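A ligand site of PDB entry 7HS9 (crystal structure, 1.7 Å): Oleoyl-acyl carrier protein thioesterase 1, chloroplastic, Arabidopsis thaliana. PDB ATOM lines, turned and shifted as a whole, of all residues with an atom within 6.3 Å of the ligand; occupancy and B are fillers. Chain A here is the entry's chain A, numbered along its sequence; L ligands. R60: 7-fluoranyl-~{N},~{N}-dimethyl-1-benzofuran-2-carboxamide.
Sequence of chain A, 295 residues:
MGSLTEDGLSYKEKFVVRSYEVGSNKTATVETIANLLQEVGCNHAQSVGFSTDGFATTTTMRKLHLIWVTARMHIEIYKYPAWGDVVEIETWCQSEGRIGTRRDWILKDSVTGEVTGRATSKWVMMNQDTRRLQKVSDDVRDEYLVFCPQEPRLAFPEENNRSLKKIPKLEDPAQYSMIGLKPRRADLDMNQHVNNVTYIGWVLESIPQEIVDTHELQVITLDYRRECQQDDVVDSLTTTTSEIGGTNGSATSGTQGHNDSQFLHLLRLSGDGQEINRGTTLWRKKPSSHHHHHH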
ATOM      1  N   GLY A  41     -10.960  10.037 -25.354  1.00  0.00           N
ATOM      2  CA  GLY A  41     -11.332  10.716 -24.107  1.00  0.00           C
ATOM      3  C   GLY A  41     -10.143  10.751 -23.148  1.00  0.00           C
ATOM      4  O   GLY A  41      -9.869  11.796 -22.539  1.00  0.00           O
ATOM      5  N   HIS A  44      -7.529  13.267 -24.369  1.00  0.00           N
ATOM      6  CA  HIS A  44      -8.009  14.620 -24.111  1.00  0.00           C
ATOM      7  C   HIS A  44      -7.689  14.990 -22.623  1.00  0.00           C
ATOM      8  O   HIS A  44      -7.110  16.045 -22.365  1.00  0.00           O
ATOM      9  CB  HIS A  44      -9.531  14.724 -24.361  1.00  0.00           C
ATOM     10  CG  HIS A  44     -10.098  16.100 -24.248  1.00  0.00           C
ATOM     11  ND1 HIS A  44     -11.466  16.324 -24.178  1.00  0.00           N
ATOM     12  CD2 HIS A  44      -9.463  17.310 -24.201  1.00  0.00           C
ATOM     13  CE1 HIS A  44     -11.623  17.642 -24.115  1.00  0.00           C
ATOM     14  NE2 HIS A  44     -10.442  18.275 -24.118  1.00  0.00           N
ATOM     15  N   ALA A  45      -8.012  14.084 -21.675  1.00  0.00           N
ATOM     16  CA  ALA A  45      -7.733  14.284 -20.243  1.00  0.00           C
ATOM     17  C   ALA A  45      -6.220  14.474 -19.988  1.00  0.00           C
ATOM     18  O   ALA A  45      -5.830  15.415 -19.286  1.00  0.00           O
ATOM     19  CB  ALA A  45      -8.256  13.075 -19.433  1.00  0.00           C
ATOM     20  N   GLN A  46      -5.378  13.637 -20.597  1.00  0.00           N
ATOM     21  CA  GLN A  46      -3.931  13.746 -20.456  1.00  0.00           C
ATOM     22  C   GLN A  46      -3.417  15.104 -20.949  1.00  0.00           C
ATOM     23  O   GLN A  46      -2.567  15.724 -20.299  1.00  0.00           O
ATOM     24  CB  GLN A  46      -3.252  12.575 -21.210  1.00  0.00           C
ATOM     25  CG  GLN A  46      -1.766  12.725 -21.546  1.00  0.00           C
ATOM     26  CD  GLN A  46      -0.879  12.979 -20.355  1.00  0.00           C
ATOM     27  OE1 GLN A  46      -0.998  12.339 -19.301  1.00  0.00           O
ATOM     28  NE2 GLN A  46       0.043  13.945 -20.506  1.00  0.00           N
ATOM     29  N   SER A  47      -3.946  15.563 -22.086  1.00  0.00           N
ATOM     30  CA  SER A  47      -3.516  16.797 -22.727  1.00  0.00           C
ATOM     31  C   SER A  47      -3.688  18.027 -21.854  1.00  0.00           C
ATOM     32  O   SER A  47      -2.969  18.987 -22.043  1.00  0.00           O
ATOM     33  CB  SER A  47      -4.204  17.002 -24.078  1.00  0.00           C
ATOM     34  OG  SER A  47      -5.521  17.500 -23.953  1.00  0.00           O
ATOM     35  N   VAL A  48      -4.654  18.013 -20.915  1.00  0.00           N
ATOM     36  CA  VAL A  48      -4.894  19.186 -20.064  1.00  0.00           C
ATOM     37  C   VAL A  48      -4.571  18.950 -18.571  1.00  0.00           C
ATOM     38  O   VAL A  48      -4.822  19.845 -17.753  1.00  0.00           O
ATOM     39  CB  VAL A  48      -6.313  19.743 -20.253  1.00  0.00           C
ATOM     40  CG1 VAL A  48      -6.484  20.342 -21.645  1.00  0.00           C
ATOM     41  CG2 VAL A  48      -7.372  18.683 -19.962  1.00  0.00           C
ATOM     42  N   PHE A  50      -5.605  16.193 -16.383  1.00  0.00           N
ATOM     43  CA  PHE A  50      -6.450  15.367 -15.502  1.00  0.00           C
ATOM     44  C   PHE A  50      -5.873  13.935 -15.453  1.00  0.00           C
ATOM     45  O   PHE A  50      -4.974  13.598 -16.242  1.00  0.00           O
ATOM     46  CB  PHE A  50      -7.925  15.385 -15.953  1.00  0.00           C
ATOM     47  CG  PHE A  50      -8.540  16.760 -15.865  1.00  0.00           C
ATOM     48  CD1 PHE A  50      -8.560  17.452 -14.673  1.00  0.00           C
ATOM     49  CD2 PHE A  50      -9.088  17.360 -16.982  1.00  0.00           C
ATOM     50  CE1 PHE A  50      -9.092  18.740 -14.605  1.00  0.00           C
ATOM     51  CE2 PHE A  50      -9.628  18.639 -16.907  1.00  0.00           C
ATOM     52  CZ  PHE A  50      -9.612  19.328 -15.723  1.00  0.00           C
ATOM     53  N   GLY A  54      -9.147   6.640 -16.756  1.00  0.00           N
ATOM     54  CA  GLY A  54     -10.545   6.484 -17.128  1.00  0.00           C
ATOM     55  C   GLY A  54     -11.465   7.328 -16.260  1.00  0.00           C
ATOM     56  O   GLY A  54     -12.633   7.522 -16.624  1.00  0.00           O
ATOM     57  N   PHE A  55     -10.980   7.837 -15.106  1.00  0.00           N
ATOM     58  CA  PHE A  55     -11.808   8.644 -14.222  1.00  0.00           C
ATOM     59  C   PHE A  55     -11.657  10.173 -14.439  1.00  0.00           C
ATOM     60  O   PHE A  55     -12.494  10.917 -13.940  1.00  0.00           O
ATOM     61  CB  PHE A  55     -11.601   8.253 -12.753  1.00  0.00           C
ATOM     62  CG  PHE A  55     -11.774   6.774 -12.460  1.00  0.00           C
ATOM     63  CD1 PHE A  55     -12.991   6.158 -12.644  1.00  0.00           C
ATOM     64  CD2 PHE A  55     -10.733   6.034 -11.925  1.00  0.00           C
ATOM     65  CE1 PHE A  55     -13.160   4.805 -12.354  1.00  0.00           C
ATOM     66  CE2 PHE A  55     -10.904   4.679 -11.626  1.00  0.00           C
ATOM     67  CZ  PHE A  55     -12.110   4.082 -11.845  1.00  0.00           C
ATOM     68  N   ALA A  56     -10.610  10.641 -15.150  1.00  0.00           N
ATOM     69  CA  ALA A  56     -10.392  12.064 -15.447  1.00  0.00           C
ATOM     70  C   ALA A  56     -10.592  12.987 -14.218  1.00  0.00           C
ATOM     71  O   ALA A  56     -11.339  13.954 -14.275  1.00  0.00           O
ATOM     72  CB  ALA A  56     -11.280  12.503 -16.606  1.00  0.00           C
ATOM     73  N   THR A  57      -9.944  12.653 -13.108  1.00  0.00           N
ATOM     74  CA  THR A  57     -10.063  13.386 -11.848  1.00  0.00           C
ATOM     75  C   THR A  57      -9.051  14.526 -11.699  1.00  0.00           C
ATOM     76  O   THR A  57      -8.054  14.578 -12.436  1.00  0.00           O
ATOM     77  CB  THR A  57      -9.885  12.402 -10.676  1.00  0.00           C
ATOM     78  OG1 THR A  57      -8.543  11.937 -10.685  1.00  0.00           O
ATOM     79  CG2 THR A  57     -10.865  11.255 -10.699  1.00  0.00           C
ATOM     80  N   TRP A  68     -15.216  10.062 -11.397  1.00  0.00           N
ATOM     81  CA  TRP A  68     -16.314  10.230 -12.329  1.00  0.00           C
ATOM     82  C   TRP A  68     -16.641   8.834 -12.860  1.00  0.00           C
ATOM     83  O   TRP A  68     -15.725   8.086 -13.207  1.00  0.00           O
ATOM     84  CB  TRP A  68     -15.902  11.132 -13.492  1.00  0.00           C
ATOM     85  CG  TRP A  68     -15.641  12.562 -13.112  1.00  0.00           C
ATOM     86  CD1 TRP A  68     -14.437  13.171 -12.953  1.00  0.00           C
ATOM     87  CD2 TRP A  68     -16.640  13.564 -12.884  1.00  0.00           C
ATOM     88  NE1 TRP A  68     -14.614  14.503 -12.646  1.00  0.00           N
ATOM     89  CE2 TRP A  68     -15.961  14.770 -12.593  1.00  0.00           C
ATOM     90  CE3 TRP A  68     -18.045  13.565 -12.894  1.00  0.00           C
ATOM     91  CZ2 TRP A  68     -16.641  15.957 -12.337  1.00  0.00           C
ATOM     92  CZ3 TRP A  68     -18.703  14.749 -12.647  1.00  0.00           C
ATOM     93  CH2 TRP A  68     -18.010  15.923 -12.345  1.00  0.00           C
ATOM     94  N   VAL A  69     -17.912   8.460 -12.901  1.00  0.00           N
ATOM     95  CA  VAL A  69     -18.319   7.178 -13.456  1.00  0.00           C
ATOM     96  C   VAL A  69     -19.424   7.421 -14.492  1.00  0.00           C
ATOM     97  O   VAL A  69     -20.238   8.327 -14.331  1.00  0.00           O
ATOM     98  CB  VAL A  69     -18.781   6.123 -12.407  1.00  0.00           C
ATOM     99  CG1 VAL A  69     -17.719   5.870 -11.346  1.00  0.00           C
ATOM    100  CG2 VAL A  69     -20.114   6.510 -11.792  1.00  0.00           C
ATOM    101  N   CYS A  93     -16.101  18.155 -23.719  1.00  0.00           N
ATOM    102  CA  CYS A  93     -16.920  17.989 -22.521  1.00  0.00           C
ATOM    103  C   CYS A  93     -17.681  19.249 -22.176  1.00  0.00           C
ATOM    104  O   CYS A  93     -17.309  20.336 -22.583  1.00  0.00           O
ATOM    105  CB  CYS A  93     -16.055  17.550 -21.343  1.00  0.00           C
ATOM    106  SG  CYS A  93     -15.260  15.950 -21.559  1.00  0.00           S
ATOM    107  N   GLN A  94     -18.725  19.096 -21.357  1.00  0.00           N
ATOM    108  CA  GLN A  94     -19.495  20.217 -20.845  1.00  0.00           C
ATOM    109  C   GLN A  94     -19.985  19.862 -19.449  1.00  0.00           C
ATOM    110  O   GLN A  94     -20.335  18.710 -19.196  1.00  0.00           O
ATOM    111  CB  GLN A  94     -20.693  20.524 -21.743  1.00  0.00           C
ATOM    112  CG  GLN A  94     -20.317  21.190 -23.063  1.00  0.00           C
ATOM    113  CD  GLN A  94     -21.311  22.253 -23.434  1.00  0.00           C
ATOM    114  OE1 GLN A  94     -22.384  21.972 -23.997  1.00  0.00           O
ATOM    115  NE2 GLN A  94     -20.971  23.487 -23.076  1.00  0.00           N
ATOM    116  N   THR A 101     -21.310  15.760 -15.606  1.00  0.00           N
ATOM    117  CA  THR A 101     -20.711  16.262 -16.834  1.00  0.00           C
ATOM    118  C   THR A 101     -21.139  15.386 -18.032  1.00  0.00           C
ATOM    119  O   THR A 101     -21.632  14.260 -17.865  1.00  0.00           O
ATOM    120  CB  THR A 101     -19.169  16.346 -16.714  1.00  0.00           C
ATOM    121  OG1 THR A 101     -18.642  15.029 -16.612  1.00  0.00           O
ATOM    122  CG2 THR A 101     -18.703  17.193 -15.532  1.00  0.00           C
ATOM    123  N   ARG A 102     -20.913  15.901 -19.221  1.00  0.00           N
ATOM    124  CA  ARG A 102     -21.230  15.216 -20.447  1.00  0.00           C
ATOM    125  C   ARG A 102     -19.979  15.188 -21.315  1.00  0.00           C
ATOM    126  O   ARG A 102     -19.255  16.190 -21.398  1.00  0.00           O
ATOM    127  CB  ARG A 102     -22.350  15.982 -21.158  1.00  0.00           C
ATOM    128  CG  ARG A 102     -23.021  15.196 -22.285  1.00  0.00           C
ATOM    129  CD  ARG A 102     -24.035  16.040 -23.016  1.00  0.00           C
ATOM    130  NE  ARG A 102     -23.377  16.851 -24.031  1.00  0.00           N
ATOM    131  CZ  ARG A 102     -23.208  18.171 -23.964  1.00  0.00           C
ATOM    132  NH1 ARG A 102     -22.571  18.811 -24.927  1.00  0.00           N
ATOM    133  NH2 ARG A 102     -23.677  18.845 -22.915  1.00  0.00           N
ATOM    134  N   ARG A 103     -19.700  14.028 -21.960  1.00  0.00           N
ATOM    135  CA  ARG A 103     -18.622  13.981 -22.941  1.00  0.00           C
ATOM    136  C   ARG A 103     -19.296  13.616 -24.265  1.00  0.00           C
ATOM    137  O   ARG A 103     -20.053  12.634 -24.305  1.00  0.00           O
ATOM    138  CB  ARG A 103     -17.507  12.973 -22.608  1.00  0.00           C
ATOM    139  CG  ARG A 103     -16.464  12.895 -23.768  1.00  0.00           C
ATOM    140  CD  ARG A 103     -15.231  12.037 -23.444  1.00  0.00           C
ATOM    141  NE  ARG A 103     -14.307  12.674 -22.490  1.00  0.00           N
ATOM    142  CZ  ARG A 103     -13.411  13.604 -22.822  1.00  0.00           C
ATOM    143  NH1 ARG A 103     -12.594  14.097 -21.899  1.00  0.00           N
ATOM    144  NH2 ARG A 103     -13.335  14.053 -24.063  1.00  0.00           N
ATOM    145  N   TRP A 123     -21.845  11.485 -17.077  1.00  0.00           N
ATOM    146  CA  TRP A 123     -20.948  11.048 -16.022  1.00  0.00           C
ATOM    147  C   TRP A 123     -21.390  11.692 -14.697  1.00  0.00           C
ATOM    148  O   TRP A 123     -21.851  12.827 -14.670  1.00  0.00           O
ATOM    149  CB  TRP A 123     -19.507  11.482 -16.348  1.00  0.00           C
ATOM    150  CG  TRP A 123     -18.937  10.891 -17.605  1.00  0.00           C
ATOM    151  CD1 TRP A 123     -19.258  11.221 -18.891  1.00  0.00           C
ATOM    152  CD2 TRP A 123     -17.970   9.836 -17.685  1.00  0.00           C
ATOM    153  NE1 TRP A 123     -18.531  10.451 -19.772  1.00  0.00           N
ATOM    154  CE2 TRP A 123     -17.714   9.602 -19.056  1.00  0.00           C
ATOM    155  CE3 TRP A 123     -17.255   9.095 -16.735  1.00  0.00           C
ATOM    156  CZ2 TRP A 123     -16.784   8.659 -19.492  1.00  0.00           C
ATOM    157  CZ3 TRP A 123     -16.339   8.152 -17.172  1.00  0.00           C
ATOM    158  CH2 TRP A 123     -16.113   7.944 -18.538  1.00  0.00           C
ATOM    159  N   TYR A 144     -12.848  22.358 -14.230  1.00  0.00           N
ATOM    160  CA  TYR A 144     -13.176  21.805 -15.554  1.00  0.00           C
ATOM    161  C   TYR A 144     -13.650  22.840 -16.606  1.00  0.00           C
ATOM    162  O   TYR A 144     -13.376  22.693 -17.793  1.00  0.00           O
ATOM    163  CB  TYR A 144     -14.247  20.690 -15.427  1.00  0.00           C
ATOM    164  CG  TYR A 144     -13.718  19.425 -14.786  1.00  0.00           C
ATOM    165  CD1 TYR A 144     -13.053  18.464 -15.530  1.00  0.00           C
ATOM    166  CD2 TYR A 144     -13.869  19.201 -13.419  1.00  0.00           C
ATOM    167  CE1 TYR A 144     -12.537  17.317 -14.938  1.00  0.00           C
ATOM    168  CE2 TYR A 144     -13.367  18.051 -12.819  1.00  0.00           C
ATOM    169  CZ  TYR A 144     -12.716  17.108 -13.579  1.00  0.00           C
ATOM    170  OH  TYR A 144     -12.187  16.005 -12.984  1.00  0.00           O
ATOM    171  N   LEU A 145     -14.399  23.862 -16.153  1.00  0.00           N
ATOM    172  CA  LEU A 145     -15.003  24.891 -17.008  1.00  0.00           C
ATOM    173  C   LEU A 145     -14.023  25.621 -17.939  1.00  0.00           C
ATOM    174  O   LEU A 145     -14.375  25.903 -19.095  1.00  0.00           O
ATOM    175  CB  LEU A 145     -15.811  25.883 -16.171  1.00  0.00           C
ATOM    176  CG  LEU A 145     -17.177  25.335 -15.695  1.00  0.00           C
ATOM    177  CD1 LEU A 145     -17.774  26.226 -14.632  1.00  0.00           C
ATOM    178  CD2 LEU A 145     -18.150  25.248 -16.842  1.00  0.00           C
ATOM    179  N   PHE A 147     -11.706  24.357 -19.573  1.00  0.00           N
ATOM    180  CA  PHE A 147     -11.383  23.417 -20.651  1.00  0.00           C
ATOM    181  C   PHE A 147     -12.628  23.005 -21.497  1.00  0.00           C
ATOM    182  O   PHE A 147     -12.508  22.180 -22.398  1.00  0.00           O
ATOM    183  CB  PHE A 147     -10.678  22.170 -20.085  1.00  0.00           C
ATOM    184  CG  PHE A 147      -9.480  22.498 -19.236  1.00  0.00           C
ATOM    185  CD1 PHE A 147      -8.343  23.064 -19.786  1.00  0.00           C
ATOM    186  CD2 PHE A 147      -9.488  22.267 -17.872  1.00  0.00           C
ATOM    187  CE1 PHE A 147      -7.233  23.367 -18.993  1.00  0.00           C
ATOM    188  CE2 PHE A 147      -8.377  22.573 -17.088  1.00  0.00           C
ATOM    189  CZ  PHE A 147      -7.274  23.134 -17.653  1.00  0.00           C
ATOM    190  N   CYS A 148     -13.795  23.613 -21.243  1.00  0.00           N
ATOM    191  CA  CYS A 148     -15.035  23.328 -21.946  1.00  0.00           C
ATOM    192  C   CYS A 148     -15.527  24.535 -22.760  1.00  0.00           C
ATOM    193  O   CYS A 148     -15.333  25.662 -22.320  1.00  0.00           O
ATOM    194  CB  CYS A 148     -16.093  22.903 -20.939  1.00  0.00           C
ATOM    195  SG  CYS A 148     -15.666  21.416 -20.017  1.00  0.00           S
HETATM  196  C4  R60 L   1     -13.828  15.168 -18.462  1.00  0.00           C
HETATM  197  C5  R60 L   1     -14.393  16.367 -18.225  1.00  0.00           C
HETATM  198  C6  R60 L   1     -13.553  17.346 -18.850  1.00  0.00           C
HETATM  199  C7  R60 L   1     -13.603  18.737 -18.987  1.00  0.00           C
HETATM  200  C8  R60 L   1     -12.616  19.367 -19.707  1.00  0.00           C
HETATM  201  C10 R60 L   1     -11.531  17.278 -20.165  1.00  0.00           C
HETATM  202  N   R60 L   1     -15.131  13.572 -17.189  1.00  0.00           N
HETATM  203  C   R60 L   1     -15.247  14.382 -15.988  1.00  0.00           C
HETATM  204  C2  R60 L   1     -16.045  12.429 -17.237  1.00  0.00           C
HETATM  205  C3  R60 L   1     -14.271  13.788 -18.201  1.00  0.00           C
HETATM  206  O   R60 L   1     -12.652  15.307 -19.159  1.00  0.00           O
HETATM  207  C11 R60 L   1     -12.524  16.644 -19.457  1.00  0.00           C
HETATM  208  C9  R60 L   1     -11.588  18.646 -20.299  1.00  0.00           C
HETATM  209  F   R60 L   1     -10.513  16.601 -20.733  1.00  0.00           F
HETATM  210  O2  R60 L   1     -13.960  12.896 -18.992  1.00  0.00           O
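The guanidinium group (NH1) of Arg 103 sits at hydrogen-bond distance from an oxygen (O) of the ligand (3.0 Å).
An oxygen (O) of the ligand sits close to the side-chain sulfur (SG) of Cys 93, at 3.6 Å.
O of Ala 56 is in hydrogen-bond range of OH of Tyr 144.
A ring nitrogen (ND1) of His 44 sits at hydrogen-bond distance from the guanidinium group (NH2) of Arg 103 (2.9 Å).
The indole nitrogen (NE1) of Trp 68 is in hydrogen-bond range of the side-chain hydroxyl (OH) of Tyr 144 (2.9 Å).
The side-chain sulfur (SG) of Cys 93 sits close to the guanidinium group (NH1) of Arg 103 (3.3 Å).
The side-chain sulfur (SG) of Cys 148 is in hydrogen-bond range of the backbone carbonyl oxygen (O) of Cys 93, 3.2 Å away.
The backbone carbonyl oxygen (O) of Tyr 144 sits at hydrogen-bond distance from the side-chain sulfur (SG) of Cys 148 (3.4 Å).
N of Trp 123 lies within hydrogen-bond range of O of Thr 101, at 2.9 Å.
N of Phe 50 is in hydrogen-bond range of O of Ala 45, at 3.0 Å.
His 44 touches the ligand (CG to F, 3.6 Å).
CA of Ala 45 touches F of the ligand (3.7 Å).
Val 48 touches the ligand.
Phe 50 touches the ligand.
CB of Ala 56 touches O2 of the ligand (3.6 Å).
Trp 68 touches the ligand.
Thr 101 touches the ligand.
Trp 123 touches the ligand.
CD1 of Tyr 144 touches C7 of the ligand, at 3.5 Å.
Phe 147 touches the ligand (CB to C8, 3.4 Å).
Cys 148 touches the ligand.
Hydrophobic or aromatic side chains within 4 Å of the ligand: His 44, Val 48, Phe 50, Ala 56, Trp 68, Trp 123, Tyr 144 and Phe 147.
Along chain A the residues within 4 Å of the ligand span positions 44 to 148.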
